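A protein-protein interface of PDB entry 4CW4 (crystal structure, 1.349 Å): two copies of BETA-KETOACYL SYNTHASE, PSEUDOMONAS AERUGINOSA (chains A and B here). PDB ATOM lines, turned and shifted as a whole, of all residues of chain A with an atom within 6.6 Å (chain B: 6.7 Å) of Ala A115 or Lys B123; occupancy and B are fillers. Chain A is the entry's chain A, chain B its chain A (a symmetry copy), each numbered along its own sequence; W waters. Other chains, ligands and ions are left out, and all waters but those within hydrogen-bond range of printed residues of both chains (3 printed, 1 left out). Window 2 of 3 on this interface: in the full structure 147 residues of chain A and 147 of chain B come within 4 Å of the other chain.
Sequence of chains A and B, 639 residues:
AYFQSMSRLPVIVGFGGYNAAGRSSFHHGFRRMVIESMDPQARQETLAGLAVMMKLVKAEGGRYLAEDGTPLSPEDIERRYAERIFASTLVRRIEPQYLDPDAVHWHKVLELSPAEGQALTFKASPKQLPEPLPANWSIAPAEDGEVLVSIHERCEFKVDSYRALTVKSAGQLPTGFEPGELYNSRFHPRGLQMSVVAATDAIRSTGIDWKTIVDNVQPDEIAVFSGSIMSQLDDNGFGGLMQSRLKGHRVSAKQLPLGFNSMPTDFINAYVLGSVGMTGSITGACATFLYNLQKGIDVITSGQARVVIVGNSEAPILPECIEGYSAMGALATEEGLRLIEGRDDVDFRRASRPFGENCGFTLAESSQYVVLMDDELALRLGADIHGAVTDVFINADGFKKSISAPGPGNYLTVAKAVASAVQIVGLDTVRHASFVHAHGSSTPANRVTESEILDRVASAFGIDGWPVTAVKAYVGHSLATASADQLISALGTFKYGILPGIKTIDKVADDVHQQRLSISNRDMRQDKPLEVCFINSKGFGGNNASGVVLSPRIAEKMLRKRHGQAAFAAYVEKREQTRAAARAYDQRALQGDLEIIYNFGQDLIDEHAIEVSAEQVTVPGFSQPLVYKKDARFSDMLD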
ATOM      1  N   LEU A 110      19.345 -30.665  17.382  1.00  0.00           N
ATOM      2  CA  LEU A 110      17.893 -30.723  17.359  1.00  0.00           C
ATOM      3  C   LEU A 110      17.402 -29.928  16.159  1.00  0.00           C
ATOM      4  O   LEU A 110      17.526 -28.700  16.113  1.00  0.00           O
ATOM      5  CB  LEU A 110      17.339 -30.151  18.663  1.00  0.00           C
ATOM      6  CG  LEU A 110      15.823 -30.013  18.774  1.00  0.00           C
ATOM      7  CD1 LEU A 110      15.130 -31.359  18.656  1.00  0.00           C
ATOM      8  CD2 LEU A 110      15.463 -29.354  20.088  1.00  0.00           C
ATOM      9  N   GLU A 111      16.879 -30.643  15.172  1.00  0.00           N
ATOM     10  CA  GLU A 111      16.355 -30.001  13.980  1.00  0.00           C
ATOM     11  C   GLU A 111      14.917 -29.598  14.221  1.00  0.00           C
ATOM     12  O   GLU A 111      14.041 -30.454  14.307  1.00  0.00           O
ATOM     13  CB  GLU A 111      16.430 -30.947  12.782  1.00  0.00           C
ATOM     14  CG  GLU A 111      17.842 -31.334  12.402  1.00  0.00           C
ATOM     15  CD  GLU A 111      17.884 -32.311  11.240  1.00  0.00           C
ATOM     16  OE1 GLU A 111      17.451 -31.930  10.128  1.00  0.00           O
ATOM     17  OE2 GLU A 111      18.345 -33.458  11.439  1.00  0.00           O
ATOM     18  N   LEU A 112      14.679 -28.297  14.335  1.00  0.00           N
ATOM     19  CA  LEU A 112      13.324 -27.790  14.506  1.00  0.00           C
ATOM     20  C   LEU A 112      12.786 -27.304  13.194  1.00  0.00           C
ATOM     21  O   LEU A 112      13.418 -26.508  12.514  1.00  0.00           O
ATOM     22  CB  LEU A 112      13.284 -26.661  15.522  1.00  0.00           C
ATOM     23  CG  LEU A 112      13.689 -27.082  16.928  1.00  0.00           C
ATOM     24  CD1 LEU A 112      13.244 -26.034  17.921  1.00  0.00           C
ATOM     25  CD2 LEU A 112      13.118 -28.450  17.276  1.00  0.00           C
ATOM     26  N   SER A 113      11.607 -27.808  12.852  1.00  0.00           N
ATOM     27  CA  SER A 113      10.906 -27.419  11.645  1.00  0.00           C
ATOM     28  C   SER A 113       9.544 -26.874  12.025  1.00  0.00           C
ATOM     29  O   SER A 113       8.903 -27.369  12.956  1.00  0.00           O
ATOM     30  CB  SER A 113      10.725 -28.623  10.714  1.00  0.00           C
ATOM     31  OG  SER A 113      11.945 -28.965  10.073  1.00  0.00           O
ATOM     32  N   PRO A 114       9.108 -25.823  11.328  1.00  0.00           N
ATOM     33  CA  PRO A 114       7.701 -25.479  11.432  1.00  0.00           C
ATOM     34  C   PRO A 114       6.968 -26.159  10.291  1.00  0.00           C
ATOM     35  O   PRO A 114       7.587 -26.584   9.315  1.00  0.00           O
ATOM     36  CB  PRO A 114       7.705 -23.963  11.267  1.00  0.00           C
ATOM     37  CG  PRO A 114       8.852 -23.705  10.368  1.00  0.00           C
ATOM     38  CD  PRO A 114       9.851 -24.829  10.534  1.00  0.00           C
ATOM     39  N   ALA A 115       5.660 -26.286  10.435  1.00  0.00           N
ATOM     40  CA  ALA A 115       4.820 -26.788   9.368  1.00  0.00           C
ATOM     41  C   ALA A 115       3.501 -26.036   9.436  1.00  0.00           C
ATOM     42  O   ALA A 115       3.375 -25.053  10.162  1.00  0.00           O
ATOM     43  CB  ALA A 115       4.611 -28.288   9.515  1.00  0.00           C
ATOM     44  N   GLU A 116       2.513 -26.508   8.695  1.00  0.00           N
ATOM     45  CA  GLU A 116       1.260 -25.779   8.556  1.00  0.00           C
ATOM     46  C   GLU A 116       0.464 -25.618   9.863  1.00  0.00           C
ATOM     47  O   GLU A 116      -0.397 -24.744   9.929  1.00  0.00           O
ATOM     48  CB  GLU A 116       0.395 -26.456   7.488  1.00  0.00           C
ATOM     49  CG  GLU A 116       1.112 -26.667   6.151  1.00  0.00           C
ATOM     50  CD  GLU A 116       0.726 -27.975   5.476  1.00  0.00           C
ATOM     51  OE1 GLU A 116      -0.469 -28.160   5.154  1.00  0.00           O
ATOM     52  OE2 GLU A 116       1.626 -28.821   5.273  1.00  0.00           O
ATOM     53  N   GLY A 117       0.781 -26.411  10.896  1.00  0.00           N
ATOM     54  CA  GLY A 117      -0.062 -26.554  12.091  1.00  0.00           C
ATOM     55  C   GLY A 117       0.091 -25.640  13.321  1.00  0.00           C
ATOM     56  O   GLY A 117      -0.911 -25.192  13.887  1.00  0.00           O
ATOM     57  N   GLN A 118       1.325 -25.397  13.759  1.00  0.00           N
ATOM     58  CA  GLN A 118       1.636 -24.557  14.930  1.00  0.00           C
ATOM     59  C   GLN A 118       2.791 -23.590  14.634  1.00  0.00           C
ATOM     60  O   GLN A 118       3.793 -23.977  14.024  1.00  0.00           O
ATOM     61  CB  GLN A 118       2.043 -25.431  16.128  1.00  0.00           C
ATOM     62  CG  GLN A 118       0.900 -26.157  16.832  1.00  0.00           C
ATOM     63  CD  GLN A 118       0.069 -25.231  17.709  1.00  0.00           C
ATOM     64  OE1 GLN A 118       0.611 -24.393  18.439  1.00  0.00           O
ATOM     65  NE2 GLN A 118      -1.252 -25.367  17.630  1.00  0.00           N
ATOM     66  N   ALA A 119       2.668 -22.340  15.075  1.00  0.00           N
ATOM     67  CA  ALA A 119       3.775 -21.387  14.927  1.00  0.00           C
ATOM     68  C   ALA A 119       4.966 -21.784  15.802  1.00  0.00           C
ATOM     69  O   ALA A 119       4.786 -22.364  16.882  1.00  0.00           O
ATOM     70  CB  ALA A 119       3.315 -19.969  15.266  1.00  0.00           C
ATOM     71  N   LEU A 120       6.176 -21.495  15.324  1.00  0.00           N
ATOM     72  CA  LEU A 120       7.396 -21.654  16.114  1.00  0.00           C
ATOM     73  C   LEU A 120       7.947 -20.269  16.423  1.00  0.00           C
ATOM     74  O   LEU A 120       8.632 -19.631  15.604  1.00  0.00           O
ATOM     75  CB  LEU A 120       8.430 -22.495  15.379  1.00  0.00           C
ATOM     76  CG  LEU A 120       9.812 -22.594  16.037  1.00  0.00           C
ATOM     77  CD1 LEU A 120       9.742 -22.825  17.539  1.00  0.00           C
ATOM     78  CD2 LEU A 120      10.599 -23.714  15.373  1.00  0.00           C
ATOM     79  N   HIS A 152      10.515 -20.205  10.199  1.00  0.00           N
ATOM     80  CA  HIS A 152       9.639 -20.698   9.126  1.00  0.00           C
ATOM     81  C   HIS A 152      10.224 -21.869   8.351  1.00  0.00           C
ATOM     82  O   HIS A 152       9.526 -22.497   7.539  1.00  0.00           O
ATOM     83  CB  HIS A 152       9.351 -19.567   8.152  1.00  0.00           C
ATOM     84  CG  HIS A 152       8.899 -18.321   8.831  1.00  0.00           C
ATOM     85  ND1 HIS A 152       7.623 -18.186   9.324  1.00  0.00           N
ATOM     86  CD2 HIS A 152       9.562 -17.199   9.190  1.00  0.00           C
ATOM     87  CE1 HIS A 152       7.506 -17.011   9.913  1.00  0.00           C
ATOM     88  NE2 HIS A 152       8.668 -16.389   9.841  1.00  0.00           N
ATOM     89  N   THR B 121       6.396 -23.991  21.176  1.00  0.00           N
ATOM     90  CA  THR B 121       6.004 -25.317  20.790  1.00  0.00           C
ATOM     91  C   THR B 121       6.622 -25.634  19.452  1.00  0.00           C
ATOM     92  O   THR B 121       6.733 -24.764  18.586  1.00  0.00           O
ATOM     93  CB  THR B 121       4.487 -25.365  20.681  1.00  0.00           C
ATOM     94  OG1 THR B 121       3.936 -24.887  21.908  1.00  0.00           O
ATOM     95  CG2 THR B 121       3.992 -26.762  20.419  1.00  0.00           C
ATOM     96  N   PHE B 122       7.028 -26.883  19.284  1.00  0.00           N
ATOM     97  CA  PHE B 122       7.613 -27.318  18.030  1.00  0.00           C
ATOM     98  C   PHE B 122       7.473 -28.817  17.902  1.00  0.00           C
ATOM     99  O   PHE B 122       7.241 -29.517  18.897  1.00  0.00           O
ATOM    100  CB  PHE B 122       9.080 -26.898  17.940  1.00  0.00           C
ATOM    101  CG  PHE B 122       9.916 -27.370  19.097  1.00  0.00           C
ATOM    102  CD1 PHE B 122      10.494 -28.629  19.087  1.00  0.00           C
ATOM    103  CD2 PHE B 122      10.130 -26.550  20.198  1.00  0.00           C
ATOM    104  CE1 PHE B 122      11.265 -29.064  20.148  1.00  0.00           C
ATOM    105  CE2 PHE B 122      10.886 -26.982  21.257  1.00  0.00           C
ATOM    106  CZ  PHE B 122      11.462 -28.235  21.238  1.00  0.00           C
ATOM    107  N   LYS B 123       7.581 -29.307  16.676  1.00  0.00           N
ATOM    108  CA  LYS B 123       7.651 -30.743  16.470  1.00  0.00           C
ATOM    109  C   LYS B 123       9.095 -31.139  16.281  1.00  0.00           C
ATOM    110  O   LYS B 123       9.914 -30.366  15.771  1.00  0.00           O
ATOM    111  CB  LYS B 123       6.814 -31.186  15.278  1.00  0.00           C
ATOM    112  CG  LYS B 123       7.392 -30.841  13.941  1.00  0.00           C
ATOM    113  CD  LYS B 123       6.323 -30.994  12.878  1.00  0.00           C
ATOM    114  CE  LYS B 123       6.908 -31.059  11.485  1.00  0.00           C
ATOM    115  NZ  LYS B 123       5.823 -31.332  10.501  1.00  0.00           N
ATOM    116  N   ALA B 124       9.398 -32.353  16.711  1.00  0.00           N
ATOM    117  CA  ALA B 124      10.761 -32.839  16.669  1.00  0.00           C
ATOM    118  C   ALA B 124      10.791 -34.345  16.619  1.00  0.00           C
ATOM    119  O   ALA B 124       9.847 -35.010  17.011  1.00  0.00           O
ATOM    120  CB  ALA B 124      11.507 -32.368  17.878  1.00  0.00           C
ATOM    121  N   SER B 125      11.907 -34.875  16.133  1.00  0.00           N
ATOM    122  CA  SER B 125      12.196 -36.293  16.215  1.00  0.00           C
ATOM    123  C   SER B 125      12.572 -36.609  17.662  1.00  0.00           C
ATOM    124  O   SER B 125      13.465 -35.970  18.219  1.00  0.00           O
ATOM    125  CB  SER B 125      13.362 -36.643  15.289  1.00  0.00           C
ATOM    126  OG  SER B 125      13.156 -36.117  13.991  1.00  0.00           O
ATOM    127  N   ALA B 142       2.746 -37.285  17.926  1.00  0.00           N
ATOM    128  CA  ALA B 142       2.423 -36.597  16.685  1.00  0.00           C
ATOM    129  C   ALA B 142       2.557 -37.566  15.517  1.00  0.00           C
ATOM    130  O   ALA B 142       2.827 -38.759  15.706  1.00  0.00           O
ATOM    131  CB  ALA B 142       3.322 -35.384  16.496  1.00  0.00           C
ATOM    132  N   GLU B 143       2.352 -37.047  14.311  1.00  0.00           N
ATOM    133  CA  GLU B 143       2.379 -37.869  13.111  1.00  0.00           C
ATOM    134  C   GLU B 143       3.814 -38.160  12.682  1.00  0.00           C
ATOM    135  O   GLU B 143       4.735 -37.410  13.007  1.00  0.00           O
ATOM    136  CB  GLU B 143       1.620 -37.156  11.983  1.00  0.00           C
ATOM    137  CG  GLU B 143       1.641 -37.885  10.644  1.00  0.00           C
ATOM    138  CD  GLU B 143       0.922 -37.122   9.544  1.00  0.00           C
ATOM    139  OE1 GLU B 143       0.473 -35.984   9.808  1.00  0.00           O
ATOM    140  OE2 GLU B 143       0.812 -37.659   8.418  1.00  0.00           O
ATOM    141  N   GLU B 146       7.190 -38.378  14.863  1.00  0.00           N
ATOM    142  CA  GLU B 146       7.637 -37.189  15.582  1.00  0.00           C
ATOM    143  C   GLU B 146       6.781 -36.955  16.816  1.00  0.00           C
ATOM    144  O   GLU B 146       5.756 -37.611  17.005  1.00  0.00           O
ATOM    145  CB  GLU B 146       7.605 -35.966  14.673  1.00  0.00           C
ATOM    146  CG  GLU B 146       8.362 -36.171  13.382  1.00  0.00           C
ATOM    147  CD  GLU B 146       9.173 -34.961  12.983  1.00  0.00           C
ATOM    148  OE1 GLU B 146       8.564 -33.923  12.645  1.00  0.00           O
ATOM    149  OE2 GLU B 146      10.422 -35.053  13.007  1.00  0.00           O
ATOM    150  N   VAL B 147       7.223 -36.029  17.662  1.00  0.00           N
ATOM    151  CA  VAL B 147       6.472 -35.653  18.856  1.00  0.00           C
ATOM    152  C   VAL B 147       6.288 -34.144  18.907  1.00  0.00           C
ATOM    153  O   VAL B 147       7.059 -33.390  18.315  1.00  0.00           O
ATOM    154  CB  VAL B 147       7.165 -36.114  20.166  1.00  0.00           C
ATOM    155  CG1 VAL B 147       7.153 -37.637  20.274  1.00  0.00           C
ATOM    156  CG2 VAL B 147       8.590 -35.564  20.265  1.00  0.00           C
ATOM    157  N   LEU B 148       5.259 -33.726  19.633  1.00  0.00           N
ATOM    158  CA  LEU B 148       4.949 -32.313  19.816  1.00  0.00           C
ATOM    159  C   LEU B 148       5.474 -31.862  21.172  1.00  0.00           C
ATOM    160  O   LEU B 148       5.056 -32.361  22.204  1.00  0.00           O
ATOM    161  CB  LEU B 148       3.443 -32.093  19.722  1.00  0.00           C
ATOM    162  CG  LEU B 148       2.981 -30.638  19.802  1.00  0.00           C
ATOM    163  CD1 LEU B 148       3.545 -29.795  18.655  1.00  0.00           C
ATOM    164  CD2 LEU B 148       1.446 -30.574  19.822  1.00  0.00           C
ATOM    165  N   VAL B 149       6.409 -30.926  21.162  1.00  0.00           N
ATOM    166  CA  VAL B 149       7.071 -30.483  22.379  1.00  0.00           C
ATOM    167  C   VAL B 149       6.657 -29.066  22.727  1.00  0.00           C
ATOM    168  O   VAL B 149       6.568 -28.216  21.850  1.00  0.00           O
ATOM    169  CB  VAL B 149       8.594 -30.484  22.178  1.00  0.00           C
ATOM    170  CG1 VAL B 149       9.305 -30.109  23.459  1.00  0.00           C
ATOM    171  CG2 VAL B 149       9.041 -31.852  21.688  1.00  0.00           C
HETATM  172  O   HOH W   1       6.046 -21.688  19.315  1.00  0.00           O
HETATM  173  O   HOH W   2      13.905 -33.118  15.103  1.00  0.00           O
HETATM  174  O   HOH W   3      11.145 -30.533  13.454  1.00  0.00           O
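Water W3 lies within hydrogen-bond range of O of Lys B123 (2.6 Å), N of Ser A113 (2.8 Å) and O of Glu A111 (3.0 Å). Water W2 lies within hydrogen-bond range of O of Glu A111 (2.8 Å) and N of Ser B125 (2.9 Å). Water W1 bridges the backbone carbonyl oxygen (O) of Ala A119 (2.8 Å) and the backbone NH (N) of Thr B121 (3.0 Å).
O of Phe B122 lies within hydrogen-bond range of N of Val B149, 2.8 Å away. The backbone NH of Val B147 lies within hydrogen-bond range of the backbone carbonyl oxygen of Ala B124, 2.9 Å away.
No position is printed for both chains. Of the 6 pairs that touch across the chains among the printed residues, none has its exchanged pair printed and touching as well.
Among the printed residues, merely in contact across the chains: Leu A112 with Phe B122 (3.2 Å), Ala A115 with Lys B123 (3.4 Å), Ala A119 with Thr B121 (3.5 Å), Leu A120 with Thr B121 (3.7 Å), Leu A110 with Ala B124 (3.8 Å) and Ser A113 with Lys B123 (3.9 Å).
Ala A115 touches just one residue of chain B: Lys B123. Of chain A, only Ser A113 (3.9 Å) and Ala A115 (3.4 Å) come within 4 Å of Lys B123. Printed residues of chain B within 4 Å of Leu A120: Thr B121 (3.7 Å). Printed residues of chain B within 4 Å of Leu A110: Ala B124 (3.8 Å). Of the printed residues of chain B, Ser A113 touches Lys B123 (3.9 Å). The nearest residue of chain A that does not touch Lys B123 is Leu A112 (4.03 Å). The nearest printed residue of chain A that does not touch Ala B124 is Leu A112 (4.3 Å).
Of the 12 printed residues of chain A, 6 touch a printed residue of chain B. Printed residues of chain A that touch a printed residue of chain B: Leu A110, Leu A112, Ser A113, Ala A115, Ala A119 and Leu A120. Hydrophobic or aromatic side chains of chain A within 4 Å of the printed part of chain B: Leu A110, Leu A112, Ala A115 and Leu A120. Hydrophobic or aromatic side chains of chain B that line the printed part of chain A: Phe B122 and Ala B124. Among the printed residues, no Asp or Glu carboxylate lies within 4 Å of a Lys or Arg side-chain nitrogen of the other chain.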
